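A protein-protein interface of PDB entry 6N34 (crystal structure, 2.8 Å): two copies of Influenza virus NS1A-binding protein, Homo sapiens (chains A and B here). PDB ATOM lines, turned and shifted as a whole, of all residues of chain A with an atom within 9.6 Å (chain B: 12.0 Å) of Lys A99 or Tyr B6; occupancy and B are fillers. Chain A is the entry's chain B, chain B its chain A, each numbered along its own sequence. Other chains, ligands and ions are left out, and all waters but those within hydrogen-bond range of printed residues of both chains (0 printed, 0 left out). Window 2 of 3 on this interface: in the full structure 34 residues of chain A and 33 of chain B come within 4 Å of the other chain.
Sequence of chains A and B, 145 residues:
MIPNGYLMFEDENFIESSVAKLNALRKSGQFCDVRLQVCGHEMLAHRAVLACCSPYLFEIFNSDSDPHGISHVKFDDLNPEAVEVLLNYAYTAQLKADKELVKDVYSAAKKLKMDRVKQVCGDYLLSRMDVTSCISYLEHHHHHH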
ATOM      1  N   VAL A  85      13.517  20.686 -17.411  1.00  0.00           N
ATOM      2  CA  VAL A  85      14.509  19.622 -17.454  1.00  0.00           C
ATOM      3  C   VAL A  85      14.657  19.093 -18.876  1.00  0.00           C
ATOM      4  O   VAL A  85      15.771  18.861 -19.362  1.00  0.00           O
ATOM      5  CB  VAL A  85      14.131  18.504 -16.463  1.00  0.00           C
ATOM      6  CG1 VAL A  85      15.146  17.394 -16.499  1.00  0.00           C
ATOM      7  CG2 VAL A  85      14.053  19.056 -15.077  1.00  0.00           C
ATOM      8  N   LEU A  95      20.612  15.244 -18.188  1.00  0.00           N
ATOM      9  CA  LEU A  95      19.277  15.218 -17.587  1.00  0.00           C
ATOM     10  C   LEU A  95      19.434  15.195 -16.084  1.00  0.00           C
ATOM     11  O   LEU A  95      20.007  14.263 -15.561  1.00  0.00           O
ATOM     12  CB  LEU A  95      18.550  13.981 -18.087  1.00  0.00           C
ATOM     13  CG  LEU A  95      17.043  14.118 -18.084  1.00  0.00           C
ATOM     14  CD1 LEU A  95      16.463  13.554 -19.349  1.00  0.00           C
ATOM     15  CD2 LEU A  95      16.467  13.415 -16.891  1.00  0.00           C
ATOM     16  N   LYS A  96      18.963  16.241 -15.437  1.00  0.00           N
ATOM     17  CA  LYS A  96      19.080  16.310 -13.972  1.00  0.00           C
ATOM     18  C   LYS A  96      17.668  16.462 -13.450  1.00  0.00           C
ATOM     19  O   LYS A  96      16.966  17.313 -13.933  1.00  0.00           O
ATOM     20  CB  LYS A  96      19.975  17.481 -13.576  1.00  0.00           C
ATOM     21  CG  LYS A  96      21.216  17.641 -14.436  1.00  0.00           C
ATOM     22  CD  LYS A  96      21.210  18.892 -15.278  1.00  0.00           C
ATOM     23  CE  LYS A  96      22.601  19.382 -15.606  1.00  0.00           C
ATOM     24  NZ  LYS A  96      22.584  20.445 -16.633  1.00  0.00           N
ATOM     25  N   ALA A  97      17.297  15.607 -12.522  1.00  0.00           N
ATOM     26  CA  ALA A  97      15.960  15.568 -11.948  1.00  0.00           C
ATOM     27  C   ALA A  97      15.998  14.969 -10.551  1.00  0.00           C
ATOM     28  O   ALA A  97      16.738  14.018 -10.296  1.00  0.00           O
ATOM     29  CB  ALA A  97      15.001  14.760 -12.831  1.00  0.00           C
ATOM     30  N   ASP A  98      15.191  15.522  -9.652  1.00  0.00           N
ATOM     31  CA  ASP A  98      15.056  14.914  -8.341  1.00  0.00           C
ATOM     32  C   ASP A  98      14.207  13.653  -8.443  1.00  0.00           C
ATOM     33  O   ASP A  98      13.447  13.461  -9.396  1.00  0.00           O
ATOM     34  CB  ASP A  98      14.439  15.897  -7.343  1.00  0.00           C
ATOM     35  CG  ASP A  98      14.682  15.492  -5.888  1.00  0.00           C
ATOM     36  OD1 ASP A  98      15.301  14.423  -5.666  1.00  0.00           O
ATOM     37  OD2 ASP A  98      14.269  16.243  -4.969  1.00  0.00           O
ATOM     38  N   LYS A  99      14.357  12.784  -7.440  1.00  0.00           N
ATOM     39  CA  LYS A  99      13.610  11.530  -7.391  1.00  0.00           C
ATOM     40  C   LYS A  99      12.110  11.748  -7.609  1.00  0.00           C
ATOM     41  O   LYS A  99      11.485  11.049  -8.414  1.00  0.00           O
ATOM     42  CB  LYS A  99      13.865  10.822  -6.053  1.00  0.00           C
ATOM     43  CG  LYS A  99      15.256  10.185  -5.886  1.00  0.00           C
ATOM     44  CD  LYS A  99      15.412   9.482  -4.518  1.00  0.00           C
ATOM     45  CE  LYS A  99      16.579   8.471  -4.469  1.00  0.00           C
ATOM     46  NZ  LYS A  99      17.852   9.039  -3.923  1.00  0.00           N
ATOM     47  N   GLU A 100      11.510  12.725  -6.913  1.00  0.00           N
ATOM     48  CA  GLU A 100      10.059  12.908  -6.992  1.00  0.00           C
ATOM     49  C   GLU A 100       9.609  13.627  -8.257  1.00  0.00           C
ATOM     50  O   GLU A 100       8.414  13.608  -8.576  1.00  0.00           O
ATOM     51  CB  GLU A 100       9.537  13.682  -5.782  1.00  0.00           C
ATOM     52  CG  GLU A 100       9.688  15.188  -5.892  1.00  0.00           C
ATOM     53  CD  GLU A 100      11.007  15.669  -5.334  1.00  0.00           C
ATOM     54  OE1 GLU A 100      11.849  14.806  -5.014  1.00  0.00           O
ATOM     55  OE2 GLU A 100      11.193  16.901  -5.199  1.00  0.00           O
ATOM     56  N   LEU A 101      10.525  14.274  -8.971  1.00  0.00           N
ATOM     57  CA  LEU A 101      10.179  14.906 -10.236  1.00  0.00           C
ATOM     58  C   LEU A 101      10.130  13.909 -11.389  1.00  0.00           C
ATOM     59  O   LEU A 101       9.433  14.157 -12.382  1.00  0.00           O
ATOM     60  CB  LEU A 101      11.195  16.003 -10.551  1.00  0.00           C
ATOM     61  CG  LEU A 101      10.752  17.111 -11.510  1.00  0.00           C
ATOM     62  CD1 LEU A 101       9.493  17.753 -10.986  1.00  0.00           C
ATOM     63  CD2 LEU A 101      11.841  18.152 -11.703  1.00  0.00           C
ATOM     64  N   VAL A 102      10.839  12.784 -11.260  1.00  0.00           N
ATOM     65  CA  VAL A 102      11.069  11.875 -12.376  1.00  0.00           C
ATOM     66  C   VAL A 102       9.768  11.364 -12.967  1.00  0.00           C
ATOM     67  O   VAL A 102       9.680  11.153 -14.181  1.00  0.00           O
ATOM     68  CB  VAL A 102      11.993  10.722 -11.926  1.00  0.00           C
ATOM     69  CG1 VAL A 102      12.071   9.611 -12.964  1.00  0.00           C
ATOM     70  CG2 VAL A 102      13.387  11.258 -11.652  1.00  0.00           C
ATOM     71  N   LYS A 103       8.739  11.158 -12.146  1.00  0.00           N
ATOM     72  CA  LYS A 103       7.452  10.748 -12.697  1.00  0.00           C
ATOM     73  C   LYS A 103       6.973  11.725 -13.767  1.00  0.00           C
ATOM     74  O   LYS A 103       6.550  11.317 -14.853  1.00  0.00           O
ATOM     75  CB  LYS A 103       6.417  10.620 -11.575  1.00  0.00           C
ATOM     76  CG  LYS A 103       5.040  10.181 -12.056  1.00  0.00           C
ATOM     77  CD  LYS A 103       5.144   9.079 -13.130  1.00  0.00           C
ATOM     78  CE  LYS A 103       3.846   8.948 -13.931  1.00  0.00           C
ATOM     79  NZ  LYS A 103       3.866   7.851 -14.937  1.00  0.00           N
ATOM     80  N   ASP A 104       7.079  13.025 -13.495  1.00  0.00           N
ATOM     81  CA  ASP A 104       6.522  14.026 -14.398  1.00  0.00           C
ATOM     82  C   ASP A 104       7.359  14.201 -15.658  1.00  0.00           C
ATOM     83  O   ASP A 104       6.815  14.500 -16.730  1.00  0.00           O
ATOM     84  CB  ASP A 104       6.387  15.347 -13.656  1.00  0.00           C
ATOM     85  CG  ASP A 104       5.192  15.359 -12.744  1.00  0.00           C
ATOM     86  OD1 ASP A 104       4.515  14.311 -12.666  1.00  0.00           O
ATOM     87  OD2 ASP A 104       4.920  16.405 -12.120  1.00  0.00           O
ATOM     88  N   VAL A 105       8.682  14.046 -15.550  1.00  0.00           N
ATOM     89  CA  VAL A 105       9.519  14.167 -16.735  1.00  0.00           C
ATOM     90  C   VAL A 105       9.262  12.994 -17.655  1.00  0.00           C
ATOM     91  O   VAL A 105       9.468  13.086 -18.870  1.00  0.00           O
ATOM     92  CB  VAL A 105      11.001  14.284 -16.338  1.00  0.00           C
ATOM     93  CG1 VAL A 105      11.183  15.417 -15.377  1.00  0.00           C
ATOM     94  CG2 VAL A 105      11.423  13.062 -15.679  1.00  0.00           C
ATOM     95  N   TYR A 106       8.802  11.874 -17.096  1.00  0.00           N
ATOM     96  CA  TYR A 106       8.477  10.728 -17.925  1.00  0.00           C
ATOM     97  C   TYR A 106       7.277  11.036 -18.792  1.00  0.00           C
ATOM     98  O   TYR A 106       7.269  10.733 -19.985  1.00  0.00           O
ATOM     99  CB  TYR A 106       8.215   9.483 -17.071  1.00  0.00           C
ATOM    100  CG  TYR A 106       7.558   8.368 -17.866  1.00  0.00           C
ATOM    101  CD1 TYR A 106       8.293   7.583 -18.740  1.00  0.00           C
ATOM    102  CD2 TYR A 106       6.191   8.128 -17.765  1.00  0.00           C
ATOM    103  CE1 TYR A 106       7.680   6.591 -19.482  1.00  0.00           C
ATOM    104  CE2 TYR A 106       5.581   7.143 -18.503  1.00  0.00           C
ATOM    105  CZ  TYR A 106       6.326   6.380 -19.354  1.00  0.00           C
ATOM    106  OH  TYR A 106       5.720   5.390 -20.075  1.00  0.00           O
ATOM    107  N   CYS A 121      14.049   7.582 -18.059  1.00  0.00           N
ATOM    108  CA  CYS A 121      13.170   7.895 -16.942  1.00  0.00           C
ATOM    109  C   CYS A 121      12.311   6.706 -16.564  1.00  0.00           C
ATOM    110  O   CYS A 121      12.236   6.327 -15.397  1.00  0.00           O
ATOM    111  CB  CYS A 121      12.282   9.088 -17.273  1.00  0.00           C
ATOM    112  SG  CYS A 121      13.121  10.614 -16.981  1.00  0.00           S
ATOM    113  N   TYR A 124      14.329   4.197 -14.689  1.00  0.00           N
ATOM    114  CA  TYR A 124      14.578   4.572 -13.304  1.00  0.00           C
ATOM    115  C   TYR A 124      13.389   4.180 -12.438  1.00  0.00           C
ATOM    116  O   TYR A 124      13.544   3.531 -11.397  1.00  0.00           O
ATOM    117  CB  TYR A 124      14.875   6.074 -13.185  1.00  0.00           C
ATOM    118  CG  TYR A 124      15.146   6.523 -11.754  1.00  0.00           C
ATOM    119  CD1 TYR A 124      14.103   6.897 -10.912  1.00  0.00           C
ATOM    120  CD2 TYR A 124      16.439   6.549 -11.241  1.00  0.00           C
ATOM    121  CE1 TYR A 124      14.342   7.296  -9.613  1.00  0.00           C
ATOM    122  CE2 TYR A 124      16.686   6.945  -9.942  1.00  0.00           C
ATOM    123  CZ  TYR A 124      15.634   7.319  -9.130  1.00  0.00           C
ATOM    124  OH  TYR A 124      15.869   7.717  -7.824  1.00  0.00           O
ATOM    125  N   LEU A 125      12.182   4.508 -12.894  1.00  0.00           N
ATOM    126  CA  LEU A 125      10.991   4.249 -12.095  1.00  0.00           C
ATOM    127  C   LEU A 125      10.777   2.761 -11.882  1.00  0.00           C
ATOM    128  O   LEU A 125      10.645   2.310 -10.743  1.00  0.00           O
ATOM    129  CB  LEU A 125       9.771   4.870 -12.761  1.00  0.00           C
ATOM    130  CG  LEU A 125       9.718   6.385 -12.806  1.00  0.00           C
ATOM    131  CD1 LEU A 125       8.658   6.802 -13.795  1.00  0.00           C
ATOM    132  CD2 LEU A 125       9.407   6.919 -11.425  1.00  0.00           C
ATOM    133  N   SER A 127      12.576   0.077 -11.871  1.00  0.00           N
ATOM    134  CA  SER A 127      13.469  -0.585 -10.920  1.00  0.00           C
ATOM    135  C   SER A 127      13.006  -0.386  -9.475  1.00  0.00           C
ATOM    136  O   SER A 127      13.071  -1.327  -8.667  1.00  0.00           O
ATOM    137  CB  SER A 127      14.907  -0.092 -11.100  1.00  0.00           C
ATOM    138  OG  SER A 127      15.122   1.103 -10.373  1.00  0.00           O
ATOM    139  N   ARG A 128      12.520   0.805  -9.135  1.00  0.00           N
ATOM    140  CA  ARG A 128      11.792   0.997  -7.891  1.00  0.00           C
ATOM    141  C   ARG A 128      10.444   0.281  -7.968  1.00  0.00           C
ATOM    142  O   ARG A 128       9.690   0.251  -6.996  1.00  0.00           O
ATOM    143  CB  ARG A 128      11.581   2.483  -7.603  1.00  0.00           C
ATOM    144  CG  ARG A 128      12.820   3.246  -7.160  1.00  0.00           C
ATOM    145  CD  ARG A 128      13.654   3.754  -8.323  1.00  0.00           C
ATOM    146  NE  ARG A 128      14.920   4.314  -7.848  1.00  0.00           N
ATOM    147  CZ  ARG A 128      16.121   3.774  -8.064  1.00  0.00           C
ATOM    148  NH1 ARG A 128      16.239   2.661  -8.785  1.00  0.00           N
ATOM    149  NH2 ARG A 128      17.213   4.351  -7.561  1.00  0.00           N
ATOM    150  N   TYR B   6      18.280   9.865  -6.609  1.00  0.00           N
ATOM    151  CA  TYR B   6      18.350  11.118  -7.338  1.00  0.00           C
ATOM    152  C   TYR B   6      18.898  10.831  -8.733  1.00  0.00           C
ATOM    153  O   TYR B   6      19.897  10.126  -8.857  1.00  0.00           O
ATOM    154  CB  TYR B   6      19.225  12.117  -6.588  1.00  0.00           C
ATOM    155  CG  TYR B   6      19.321  13.452  -7.276  1.00  0.00           C
ATOM    156  CD1 TYR B   6      18.369  14.433  -7.054  1.00  0.00           C
ATOM    157  CD2 TYR B   6      20.356  13.729  -8.156  1.00  0.00           C
ATOM    158  CE1 TYR B   6      18.447  15.653  -7.684  1.00  0.00           C
ATOM    159  CE2 TYR B   6      20.443  14.944  -8.787  1.00  0.00           C
ATOM    160  CZ  TYR B   6      19.484  15.905  -8.551  1.00  0.00           C
ATOM    161  OH  TYR B   6      19.560  17.125  -9.181  1.00  0.00           O
ATOM    162  N   LEU B   7      18.273  11.372  -9.779  1.00  0.00           N
ATOM    163  CA  LEU B   7      18.449  10.863 -11.137  1.00  0.00           C
ATOM    164  C   LEU B   7      19.190  11.842 -12.030  1.00  0.00           C
ATOM    165  O   LEU B   7      18.787  13.003 -12.159  1.00  0.00           O
ATOM    166  CB  LEU B   7      17.104  10.538 -11.787  1.00  0.00           C
ATOM    167  CG  LEU B   7      17.203  10.302 -13.303  1.00  0.00           C
ATOM    168  CD1 LEU B   7      18.123   9.128 -13.637  1.00  0.00           C
ATOM    169  CD2 LEU B   7      15.833  10.092 -13.929  1.00  0.00           C
ATOM    170  N   MET B   8      20.228  11.341 -12.700  1.00  0.00           N
ATOM    171  CA  MET B   8      20.984  12.130 -13.657  1.00  0.00           C
ATOM    172  C   MET B   8      21.608  11.208 -14.692  1.00  0.00           C
ATOM    173  O   MET B   8      21.982  10.071 -14.394  1.00  0.00           O
ATOM    174  CB  MET B   8      22.062  12.963 -12.967  1.00  0.00           C
ATOM    175  CG  MET B   8      22.615  14.077 -13.836  1.00  0.00           C
ATOM    176  SD  MET B   8      23.695  15.183 -12.910  1.00  0.00           S
ATOM    177  CE  MET B   8      22.676  15.485 -11.453  1.00  0.00           C
ATOM    178  N   PHE B   9      21.726  11.718 -15.914  1.00  0.00           N
ATOM    179  CA  PHE B   9      22.166  10.910 -17.039  1.00  0.00           C
ATOM    180  C   PHE B   9      22.688  11.822 -18.141  1.00  0.00           C
ATOM    181  O   PHE B   9      22.223  12.951 -18.301  1.00  0.00           O
ATOM    182  CB  PHE B   9      21.013  10.031 -17.538  1.00  0.00           C
ATOM    183  CG  PHE B   9      21.091   9.671 -18.993  1.00  0.00           C
ATOM    184  CD1 PHE B   9      21.862   8.589 -19.416  1.00  0.00           C
ATOM    185  CD2 PHE B   9      20.370  10.396 -19.941  1.00  0.00           C
ATOM    186  CE1 PHE B   9      21.926   8.249 -20.764  1.00  0.00           C
ATOM    187  CE2 PHE B   9      20.433  10.066 -21.289  1.00  0.00           C
ATOM    188  CZ  PHE B   9      21.209   8.990 -21.702  1.00  0.00           C
ATOM    189  N   GLU B  10      23.660  11.329 -18.896  1.00  0.00           N
ATOM    190  CA  GLU B  10      24.105  12.032 -20.084  1.00  0.00           C
ATOM    191  C   GLU B  10      23.984  11.121 -21.294  1.00  0.00           C
ATOM    192  O   GLU B  10      24.330   9.942 -21.226  1.00  0.00           O
ATOM    193  CB  GLU B  10      25.535  12.531 -19.942  1.00  0.00           C
ATOM    194  CG  GLU B  10      25.942  13.448 -21.094  1.00  0.00           C
ATOM    195  CD  GLU B  10      27.344  14.026 -20.937  1.00  0.00           C
ATOM    196  OE1 GLU B  10      28.020  13.697 -19.921  1.00  0.00           O
ATOM    197  OE2 GLU B  10      27.762  14.806 -21.832  1.00  0.00           O
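The side-chain hydroxyl of Tyr A124 lies within hydrogen-bond range of the backbone NH of Tyr B6, at 3.5 Å. The backbone carbonyl oxygen of Leu B7 sits at hydrogen-bond distance from the backbone NH of Ala A97 (3.0 Å). O of Phe B9 lies within hydrogen-bond range of N of Leu A95 (2.8 Å). The side-chain amino group (NZ) of Lys A99 sits close to the backbone NH (N) of Tyr B6 (2.8 Å).
The side-chain hydroxyl (OG) of Ser A127 lies within hydrogen-bond range of the backbone carbonyl oxygen (O) of Tyr A124 (3.1 Å).
O of Leu B7 touches O of Leu A95 (3.8 Å). O of Leu A95 touches CA of Met B8, at 3.0 Å. Lys A96 touches Leu B7 (CA to O, 3.8 Å). Met B8 touches Lys A96 (SD to CG, 3.8 Å). Ala A97 touches Tyr B6 (O to CE1, 3.5 Å). Tyr B6 touches Asp A98 (CD1 to OD1, 3.4 Å). CG2 of Val A102 touches CD2 of Leu B7, at 3.5 Å. Leu B7 touches Tyr A124.
Val A85 touches none of the printed residues of chain B. Printed residues of chain B within 4 Å of Leu A95: Leu B7, Met B8 and Phe B9. Of the printed residues of chain B, Lys A96 touches Leu B7 (3.8 Å) and Met B8 (3.8 Å). Of chain B, only Tyr B6 comes within 4 Å of Lys A99. No residue of chain B comes within 4 Å of Glu A100. No residue of chain B comes within 4 Å of Leu A101. Lys A103 touches none of the printed residues of chain B. Of the printed residues of chain B, Tyr A124 touches Tyr B6 (3.5 Å) and Leu B7 (3.9 Å). Of chain A, only Ala A97, Asp A98, Lys A99 and Tyr A124 come within 4 Å of Tyr B6. Of the printed residues of chain A, Phe B9 touches Leu A95. The nearest residue of chain A that does not touch Tyr B6 is Lys A96 (4.4 Å).
Of the 5 printed residues of chain B, 4 touch a printed residue of chain A. Hydrophobic or aromatic side chains of chain B that line the printed part of chain A: Tyr B6, Leu B7 and Met B8. Of the 18 printed residues of chain A, 7 touch a printed residue of chain B. Hydrophobic or aromatic side chains of chain A within 4 Å of the printed part of chain B: Leu A95, Val A102 and Tyr A124.
No position is printed for both chains. Of the 12 pairs that touch across the chains among the printed residues, none has its exchanged pair printed and touching as well.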
